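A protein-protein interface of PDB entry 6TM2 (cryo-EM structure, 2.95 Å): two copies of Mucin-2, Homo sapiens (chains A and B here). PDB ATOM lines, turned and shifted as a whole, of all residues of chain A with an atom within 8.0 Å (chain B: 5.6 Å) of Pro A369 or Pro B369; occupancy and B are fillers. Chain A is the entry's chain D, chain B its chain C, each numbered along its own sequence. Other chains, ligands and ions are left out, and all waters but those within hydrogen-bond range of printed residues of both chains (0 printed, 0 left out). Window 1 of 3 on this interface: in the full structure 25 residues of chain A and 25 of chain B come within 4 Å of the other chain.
Thr A364 touches Phe B371, and with the chains exchanged Phe A371 touches Thr B364.
Pro A365 touches Phe B371, and with the chains exchanged Phe A371 touches Pro B365.
Pro A369 touches its own counterpart, Pro B369.
Ile A370 touches Phe B371, and with the chains exchanged Phe A371 touches Ile B370.
Of the 10 pairs that touch across the chains among the printed residues, 10 have their exchanged pair printed and touching as well.
The side-chain sulfur (SG) of Cys A343 forms a disulfide with the side-chain sulfur (SG) of Cys A368.
The side-chain hydroxyl (OG1) of Thr A364 lies within hydrogen-bond range of the backbone NH (N) of Leu A367, at 3.0 Å.
The backbone NH of Leu B367 is in hydrogen-bond range of the side-chain hydroxyl of Thr B364 (3.0 Å).
Printed residues of chain B within 4 Å of Thr A364: Phe B371.
Printed residues of chain B within 4 Å of Pro A365: Phe B371 (3.7 Å).
Pro A369 touches two residues of chain B.
Printed residues of chain B within 4 Å of Phe A371: Thr B364, Pro B365, Pro B369 and Ile B370.
Tyr A385 touches none of the printed residues of chain B.
Arg B363 touches none of the printed residues of chain A.
Of the printed residues of chain A, Thr B364 touches Phe A371.
Of the printed residues of chain A, Pro B365 touches Phe A371 (3.7 Å).
Of chain A, only Pro A369 (3.7 Å) and Phe A371 (3.6 Å) come within 4 Å of Pro B369.
The nearest printed residue of chain B that does not touch Pro A365 is Pro B369 (6.1 Å).
The backbone carbonyl oxygen (O) of Ile A370 sits close to the backbone carbonyl oxygen (O) of Ile B370 (3.2 Å).
Printed residues of chain B that touch a printed residue of chain A: Thr B364, Pro B365, Pro B369, Ile B370 and Phe B371.
Among the printed residues, pairs that only touch across the chains: Thr A364 with Phe B371 (3.8 Å), Pro A365 with Phe B371 (3.7 Å), Pro A369 with Pro B369 (3.7 Å), Pro A369 with Phe B371 (3.6 Å), Ile A370 with Phe B371 (3.1 Å), Phe A371 with Thr B364 (3.8 Å), Phe A371 with Pro B365 (3.7 Å), Phe A371 with Pro B369 (3.6 Å) and Phe A371 with Ile B370 (3.1 Å).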
ATOM      1  N   GLN A 207      10.431   8.169 -16.694  1.00  0.00           N
ATOM      2  CA  GLN A 207      11.446   7.326 -16.080  1.00  0.00           C
ATOM      3  C   GLN A 207      11.642   5.992 -16.770  1.00  0.00           C
ATOM      4  O   GLN A 207      12.417   5.176 -16.275  1.00  0.00           O
ATOM      5  CB  GLN A 207      11.119   7.048 -14.614  1.00  0.00           C
ATOM      6  CG  GLN A 207      11.347   8.180 -13.655  1.00  0.00           C
ATOM      7  CD  GLN A 207      11.057   7.749 -12.248  1.00  0.00           C
ATOM      8  OE1 GLN A 207      10.525   6.667 -12.026  1.00  0.00           O
ATOM      9  NE2 GLN A 207      11.483   8.542 -11.288  1.00  0.00           N
ATOM     10  N   CYS A 339      14.609   0.963  -0.108  1.00  0.00           N
ATOM     11  CA  CYS A 339      13.761   2.092  -0.442  1.00  0.00           C
ATOM     12  C   CYS A 339      13.607   2.273  -1.940  1.00  0.00           C
ATOM     13  O   CYS A 339      12.903   3.183  -2.366  1.00  0.00           O
ATOM     14  CB  CYS A 339      14.327   3.366   0.182  1.00  0.00           C
ATOM     15  SG  CYS A 339      14.309   3.393   1.983  1.00  0.00           S
ATOM     16  N   CYS A 343       9.581   2.145  -3.494  1.00  0.00           N
ATOM     17  CA  CYS A 343       9.051   3.224  -4.313  1.00  0.00           C
ATOM     18  C   CYS A 343       8.603   2.747  -5.680  1.00  0.00           C
ATOM     19  O   CYS A 343       7.829   3.441  -6.340  1.00  0.00           O
ATOM     20  CB  CYS A 343      10.096   4.320  -4.473  1.00  0.00           C
ATOM     21  SG  CYS A 343      10.528   5.209  -2.966  1.00  0.00           S
ATOM     22  N   TRP A 362       1.636  11.768  -4.945  1.00  0.00           N
ATOM     23  CA  TRP A 362       1.922  11.049  -3.716  1.00  0.00           C
ATOM     24  C   TRP A 362       3.330  11.242  -3.179  1.00  0.00           C
ATOM     25  O   TRP A 362       3.564  10.942  -2.007  1.00  0.00           O
ATOM     26  CB  TRP A 362       1.654   9.550  -3.912  1.00  0.00           C
ATOM     27  CG  TRP A 362       2.461   8.889  -4.975  1.00  0.00           C
ATOM     28  CD1 TRP A 362       2.150   8.787  -6.288  1.00  0.00           C
ATOM     29  CD2 TRP A 362       3.701   8.199  -4.803  1.00  0.00           C
ATOM     30  NE1 TRP A 362       3.124   8.096  -6.953  1.00  0.00           N
ATOM     31  CE2 TRP A 362       4.091   7.724  -6.061  1.00  0.00           C
ATOM     32  CE3 TRP A 362       4.529   7.952  -3.708  1.00  0.00           C
ATOM     33  CZ2 TRP A 362       5.265   7.014  -6.253  1.00  0.00           C
ATOM     34  CZ3 TRP A 362       5.691   7.252  -3.901  1.00  0.00           C
ATOM     35  CH2 TRP A 362       6.047   6.786  -5.161  1.00  0.00           C
ATOM     36  N   ARG A 363       4.261  11.741  -3.985  1.00  0.00           N
ATOM     37  CA  ARG A 363       5.643  11.883  -3.560  1.00  0.00           C
ATOM     38  C   ARG A 363       5.823  13.172  -2.776  1.00  0.00           C
ATOM     39  O   ARG A 363       5.215  14.194  -3.093  1.00  0.00           O
ATOM     40  CB  ARG A 363       6.573  11.896  -4.767  1.00  0.00           C
ATOM     41  CG  ARG A 363       6.674  10.624  -5.562  1.00  0.00           C
ATOM     42  CD  ARG A 363       7.611  10.868  -6.713  1.00  0.00           C
ATOM     43  NE  ARG A 363       7.707   9.761  -7.653  1.00  0.00           N
ATOM     44  CZ  ARG A 363       8.606   8.795  -7.597  1.00  0.00           C
ATOM     45  NH1 ARG A 363       9.513   8.787  -6.643  1.00  0.00           N
ATOM     46  NH2 ARG A 363       8.606   7.844  -8.507  1.00  0.00           N
ATOM     47  N   THR A 364       6.660  13.120  -1.750  1.00  0.00           N
ATOM     48  CA  THR A 364       7.031  14.248  -0.906  1.00  0.00           C
ATOM     49  C   THR A 364       8.549  14.260  -0.819  1.00  0.00           C
ATOM     50  O   THR A 364       9.201  13.339  -1.316  1.00  0.00           O
ATOM     51  CB  THR A 364       6.371  14.116   0.482  1.00  0.00           C
ATOM     52  OG1 THR A 364       6.745  12.883   1.092  1.00  0.00           O
ATOM     53  CG2 THR A 364       4.877  14.210   0.388  1.00  0.00           C
ATOM     54  N   PRO A 365       9.166  15.301  -0.232  1.00  0.00           N
ATOM     55  CA  PRO A 365      10.623  15.237  -0.038  1.00  0.00           C
ATOM     56  C   PRO A 365      11.087  14.213   0.977  1.00  0.00           C
ATOM     57  O   PRO A 365      12.289  13.938   1.028  1.00  0.00           O
ATOM     58  CB  PRO A 365      10.982  16.652   0.414  1.00  0.00           C
ATOM     59  CG  PRO A 365       9.963  17.473  -0.139  1.00  0.00           C
ATOM     60  CD  PRO A 365       8.718  16.698  -0.077  1.00  0.00           C
ATOM     61  N   ASP A 366      10.196  13.645   1.783  1.00  0.00           N
ATOM     62  CA  ASP A 366      10.577  12.587   2.705  1.00  0.00           C
ATOM     63  C   ASP A 366      10.193  11.203   2.217  1.00  0.00           C
ATOM     64  O   ASP A 366      10.840  10.228   2.603  1.00  0.00           O
ATOM     65  CB  ASP A 366       9.945  12.826   4.077  1.00  0.00           C
ATOM     66  CG  ASP A 366      10.537  14.022   4.781  1.00  0.00           C
ATOM     67  OD1 ASP A 366      11.727  14.318   4.557  1.00  0.00           O
ATOM     68  OD2 ASP A 366       9.805  14.677   5.548  1.00  0.00           O
ATOM     69  N   LEU A 367       9.176  11.097   1.377  1.00  0.00           N
ATOM     70  CA  LEU A 367       8.712   9.827   0.836  1.00  0.00           C
ATOM     71  C   LEU A 367       8.941   9.806  -0.664  1.00  0.00           C
ATOM     72  O   LEU A 367       8.226  10.477  -1.410  1.00  0.00           O
ATOM     73  CB  LEU A 367       7.239   9.621   1.148  1.00  0.00           C
ATOM     74  CG  LEU A 367       6.664   8.305   0.671  1.00  0.00           C
ATOM     75  CD1 LEU A 367       7.344   7.164   1.380  1.00  0.00           C
ATOM     76  CD2 LEU A 367       5.230   8.328   0.987  1.00  0.00           C
ATOM     77  N   CYS A 368       9.921   9.021  -1.092  1.00  0.00           N
ATOM     78  CA  CYS A 368      10.309   8.744  -2.472  1.00  0.00           C
ATOM     79  C   CYS A 368      10.585   9.998  -3.291  1.00  0.00           C
ATOM     80  O   CYS A 368       9.869  10.232  -4.269  1.00  0.00           O
ATOM     81  CB  CYS A 368       9.223   7.931  -3.174  1.00  0.00           C
ATOM     82  SG  CYS A 368       8.890   6.297  -2.502  1.00  0.00           S
ATOM     83  N   PRO A 369      11.595  10.809  -2.966  1.00  0.00           N
ATOM     84  CA  PRO A 369      11.776  12.071  -3.686  1.00  0.00           C
ATOM     85  C   PRO A 369      12.310  11.852  -5.090  1.00  0.00           C
ATOM     86  O   PRO A 369      12.905  10.825  -5.410  1.00  0.00           O
ATOM     87  CB  PRO A 369      12.788  12.819  -2.820  1.00  0.00           C
ATOM     88  CG  PRO A 369      13.538  11.792  -2.173  1.00  0.00           C
ATOM     89  CD  PRO A 369      12.619  10.656  -1.920  1.00  0.00           C
ATOM     90  N   ILE A 370      12.078  12.843  -5.939  1.00  0.00           N
ATOM     91  CA  ILE A 370      12.477  12.780  -7.335  1.00  0.00           C
ATOM     92  C   ILE A 370      13.238  14.060  -7.646  1.00  0.00           C
ATOM     93  O   ILE A 370      13.017  15.093  -7.016  1.00  0.00           O
ATOM     94  CB  ILE A 370      11.244  12.558  -8.252  1.00  0.00           C
ATOM     95  CG1 ILE A 370      11.658  12.174  -9.672  1.00  0.00           C
ATOM     96  CG2 ILE A 370      10.302  13.735  -8.224  1.00  0.00           C
ATOM     97  CD1 ILE A 370      10.540  11.647 -10.488  1.00  0.00           C
ATOM     98  N   PHE A 371      14.204  13.984  -8.552  1.00  0.00           N
ATOM     99  CA  PHE A 371      15.155  15.078  -8.728  1.00  0.00           C
ATOM    100  C   PHE A 371      15.172  15.480 -10.192  1.00  0.00           C
ATOM    101  O   PHE A 371      15.978  14.996 -10.985  1.00  0.00           O
ATOM    102  CB  PHE A 371      16.498  14.635  -8.141  1.00  0.00           C
ATOM    103  CG  PHE A 371      17.597  15.637  -8.217  1.00  0.00           C
ATOM    104  CD1 PHE A 371      17.420  16.932  -7.799  1.00  0.00           C
ATOM    105  CD2 PHE A 371      18.882  15.200  -8.389  1.00  0.00           C
ATOM    106  CE1 PHE A 371      18.465  17.820  -7.787  1.00  0.00           C
ATOM    107  CE2 PHE A 371      19.933  16.079  -8.340  1.00  0.00           C
ATOM    108  CZ  PHE A 371      19.715  17.388  -8.042  1.00  0.00           C
ATOM    109  N   CYS A 372      14.253  16.380 -10.541  1.00  0.00           N
ATOM    110  CA  CYS A 372      14.022  16.773 -11.923  1.00  0.00           C
ATOM    111  C   CYS A 372      14.694  18.073 -12.305  1.00  0.00           C
ATOM    112  O   CYS A 372      14.804  18.356 -13.496  1.00  0.00           O
ATOM    113  CB  CYS A 372      12.524  16.908 -12.225  1.00  0.00           C
ATOM    114  SG  CYS A 372      11.545  15.396 -12.246  1.00  0.00           S
ATOM    115  N   TYR A 385       8.577  18.048 -12.813  1.00  0.00           N
ATOM    116  CA  TYR A 385       8.002  16.743 -12.520  1.00  0.00           C
ATOM    117  C   TYR A 385       6.524  16.765 -12.843  1.00  0.00           C
ATOM    118  O   TYR A 385       5.733  17.413 -12.152  1.00  0.00           O
ATOM    119  CB  TYR A 385       8.232  16.330 -11.073  1.00  0.00           C
ATOM    120  CG  TYR A 385       7.467  15.083 -10.692  1.00  0.00           C
ATOM    121  CD1 TYR A 385       7.753  13.853 -11.265  1.00  0.00           C
ATOM    122  CD2 TYR A 385       6.498  15.127  -9.705  1.00  0.00           C
ATOM    123  CE1 TYR A 385       7.057  12.718 -10.902  1.00  0.00           C
ATOM    124  CE2 TYR A 385       5.811  14.004  -9.332  1.00  0.00           C
ATOM    125  CZ  TYR A 385       6.091  12.807  -9.932  1.00  0.00           C
ATOM    126  OH  TYR A 385       5.396  11.691  -9.557  1.00  0.00           O
ATOM    127  N   GLU A 412       4.874   8.265 -15.552  1.00  0.00           N
ATOM    128  CA  GLU A 412       5.491   9.188 -14.607  1.00  0.00           C
ATOM    129  C   GLU A 412       6.918   9.546 -14.997  1.00  0.00           C
ATOM    130  O   GLU A 412       7.686   8.695 -15.446  1.00  0.00           O
ATOM    131  CB  GLU A 412       5.485   8.528 -13.231  1.00  0.00           C
ATOM    132  CG  GLU A 412       6.124   9.295 -12.104  1.00  0.00           C
ATOM    133  CD  GLU A 412       6.043   8.549 -10.799  1.00  0.00           C
ATOM    134  OE1 GLU A 412       5.470   7.443 -10.785  1.00  0.00           O
ATOM    135  OE2 GLU A 412       6.572   9.052  -9.793  1.00  0.00           O
ATOM    136  N   ARG B 363      25.149  14.504  -5.561  1.00  0.00           N
ATOM    137  CA  ARG B 363      23.855  13.860  -5.702  1.00  0.00           C
ATOM    138  C   ARG B 363      23.463  13.780  -7.167  1.00  0.00           C
ATOM    139  O   ARG B 363      23.733  14.699  -7.944  1.00  0.00           O
ATOM    140  CB  ARG B 363      22.789  14.634  -4.939  1.00  0.00           C
ATOM    141  CG  ARG B 363      22.905  14.658  -3.440  1.00  0.00           C
ATOM    142  CD  ARG B 363      21.780  15.495  -2.898  1.00  0.00           C
ATOM    143  NE  ARG B 363      21.838  15.721  -1.462  1.00  0.00           N
ATOM    144  CZ  ARG B 363      21.237  14.972  -0.552  1.00  0.00           C
ATOM    145  NH1 ARG B 363      20.514  13.936  -0.919  1.00  0.00           N
ATOM    146  NH2 ARG B 363      21.351  15.274   0.724  1.00  0.00           N
ATOM    147  N   THR B 364      22.827  12.681  -7.544  1.00  0.00           N
ATOM    148  CA  THR B 364      22.304  12.424  -8.878  1.00  0.00           C
ATOM    149  C   THR B 364      20.865  11.964  -8.714  1.00  0.00           C
ATOM    150  O   THR B 364      20.409  11.765  -7.585  1.00  0.00           O
ATOM    151  CB  THR B 364      23.170  11.372  -9.599  1.00  0.00           C
ATOM    152  OG1 THR B 364      23.224  10.169  -8.838  1.00  0.00           O
ATOM    153  CG2 THR B 364      24.559  11.883  -9.848  1.00  0.00           C
ATOM    154  N   PRO B 365      20.090  11.817  -9.804  1.00  0.00           N
ATOM    155  CA  PRO B 365      18.746  11.245  -9.641  1.00  0.00           C
ATOM    156  C   PRO B 365      18.719   9.782  -9.251  1.00  0.00           C
ATOM    157  O   PRO B 365      17.652   9.296  -8.865  1.00  0.00           O
ATOM    158  CB  PRO B 365      18.103  11.456 -11.012  1.00  0.00           C
ATOM    159  CG  PRO B 365      18.781  12.579 -11.555  1.00  0.00           C
ATOM    160  CD  PRO B 365      20.180  12.480 -11.119  1.00  0.00           C
ATOM    161  N   ASP B 366      19.832   9.062  -9.339  1.00  0.00           N
ATOM    162  CA  ASP B 366      19.878   7.682  -8.886  1.00  0.00           C
ATOM    163  C   ASP B 366      20.533   7.521  -7.527  1.00  0.00           C
ATOM    164  O   ASP B 366      20.224   6.559  -6.822  1.00  0.00           O
ATOM    165  CB  ASP B 366      20.620   6.815  -9.904  1.00  0.00           C
ATOM    166  CG  ASP B 366      19.849   6.651 -11.190  1.00  0.00           C
ATOM    167  OD1 ASP B 366      18.603   6.670 -11.145  1.00  0.00           O
ATOM    168  OD2 ASP B 366      20.488   6.515 -12.250  1.00  0.00           O
ATOM    169  N   LEU B 367      21.408   8.436  -7.142  1.00  0.00           N
ATOM    170  CA  LEU B 367      22.100   8.394  -5.862  1.00  0.00           C
ATOM    171  C   LEU B 367      21.668   9.578  -5.016  1.00  0.00           C
ATOM    172  O   LEU B 367      22.068  10.713  -5.287  1.00  0.00           O
ATOM    173  CB  LEU B 367      23.605   8.417  -6.069  1.00  0.00           C
ATOM    174  CG  LEU B 367      24.426   8.328  -4.801  1.00  0.00           C
ATOM    175  CD1 LEU B 367      24.176   7.006  -4.121  1.00  0.00           C
ATOM    176  CD2 LEU B 367      25.835   8.447  -5.197  1.00  0.00           C
ATOM    177  N   CYS B 368      20.874   9.302  -3.992  1.00  0.00           N
ATOM    178  CA  CYS B 368      20.373  10.221  -2.973  1.00  0.00           C
ATOM    179  C   CYS B 368      19.666  11.441  -3.547  1.00  0.00           C
ATOM    180  O   CYS B 368      20.145  12.557  -3.330  1.00  0.00           O
ATOM    181  CB  CYS B 368      21.519  10.696  -2.081  1.00  0.00           C
ATOM    182  SG  CYS B 368      22.358   9.431  -1.119  1.00  0.00           S
ATOM    183  N   PRO B 369      18.538  11.299  -4.250  1.00  0.00           N
ATOM    184  CA  PRO B 369      17.933  12.464  -4.898  1.00  0.00           C
ATOM    185  C   PRO B 369      17.275  13.395  -3.893  1.00  0.00           C
ATOM    186  O   PRO B 369      16.927  13.011  -2.778  1.00  0.00           O
ATOM    187  CB  PRO B 369      16.899  11.841  -5.832  1.00  0.00           C
ATOM    188  CG  PRO B 369      16.545  10.608  -5.206  1.00  0.00           C
ATOM    189  CD  PRO B 369      17.753  10.085  -4.525  1.00  0.00           C
ATOM    190  N   ILE B 370      17.115  14.643  -4.307  1.00  0.00           N
ATOM    191  CA  ILE B 370      16.547  15.676  -3.457  1.00  0.00           C
ATOM    192  C   ILE B 370      15.443  16.358  -4.252  1.00  0.00           C
ATOM    193  O   ILE B 370      15.478  16.389  -5.480  1.00  0.00           O
ATOM    194  CB  ILE B 370      17.648  16.655  -2.966  1.00  0.00           C
ATOM    195  CG1 ILE B 370      17.144  17.550  -1.834  1.00  0.00           C
ATOM    196  CG2 ILE B 370      18.246  17.445  -4.103  1.00  0.00           C
ATOM    197  CD1 ILE B 370      18.229  18.267  -1.125  1.00  0.00           C
ATOM    198  N   PHE B 371      14.408  16.829  -3.567  1.00  0.00           N
ATOM    199  CA  PHE B 371      13.190  17.258  -4.250  1.00  0.00           C
ATOM    200  C   PHE B 371      12.857  18.672  -3.809  1.00  0.00           C
ATOM    201  O   PHE B 371      12.097  18.892  -2.867  1.00  0.00           O
ATOM    202  CB  PHE B 371      12.110  16.205  -3.994  1.00  0.00           C
ATOM    203  CG  PHE B 371      10.789  16.468  -4.631  1.00  0.00           C
ATOM    204  CD1 PHE B 371      10.683  16.791  -5.960  1.00  0.00           C
ATOM    205  CD2 PHE B 371       9.651  16.067  -3.986  1.00  0.00           C
ATOM    206  CE1 PHE B 371       9.457  16.939  -6.557  1.00  0.00           C
ATOM    207  CE2 PHE B 371       8.426  16.179  -4.594  1.00  0.00           C
ATOM    208  CZ  PHE B 371       8.338  16.619  -5.878  1.00  0.00           C
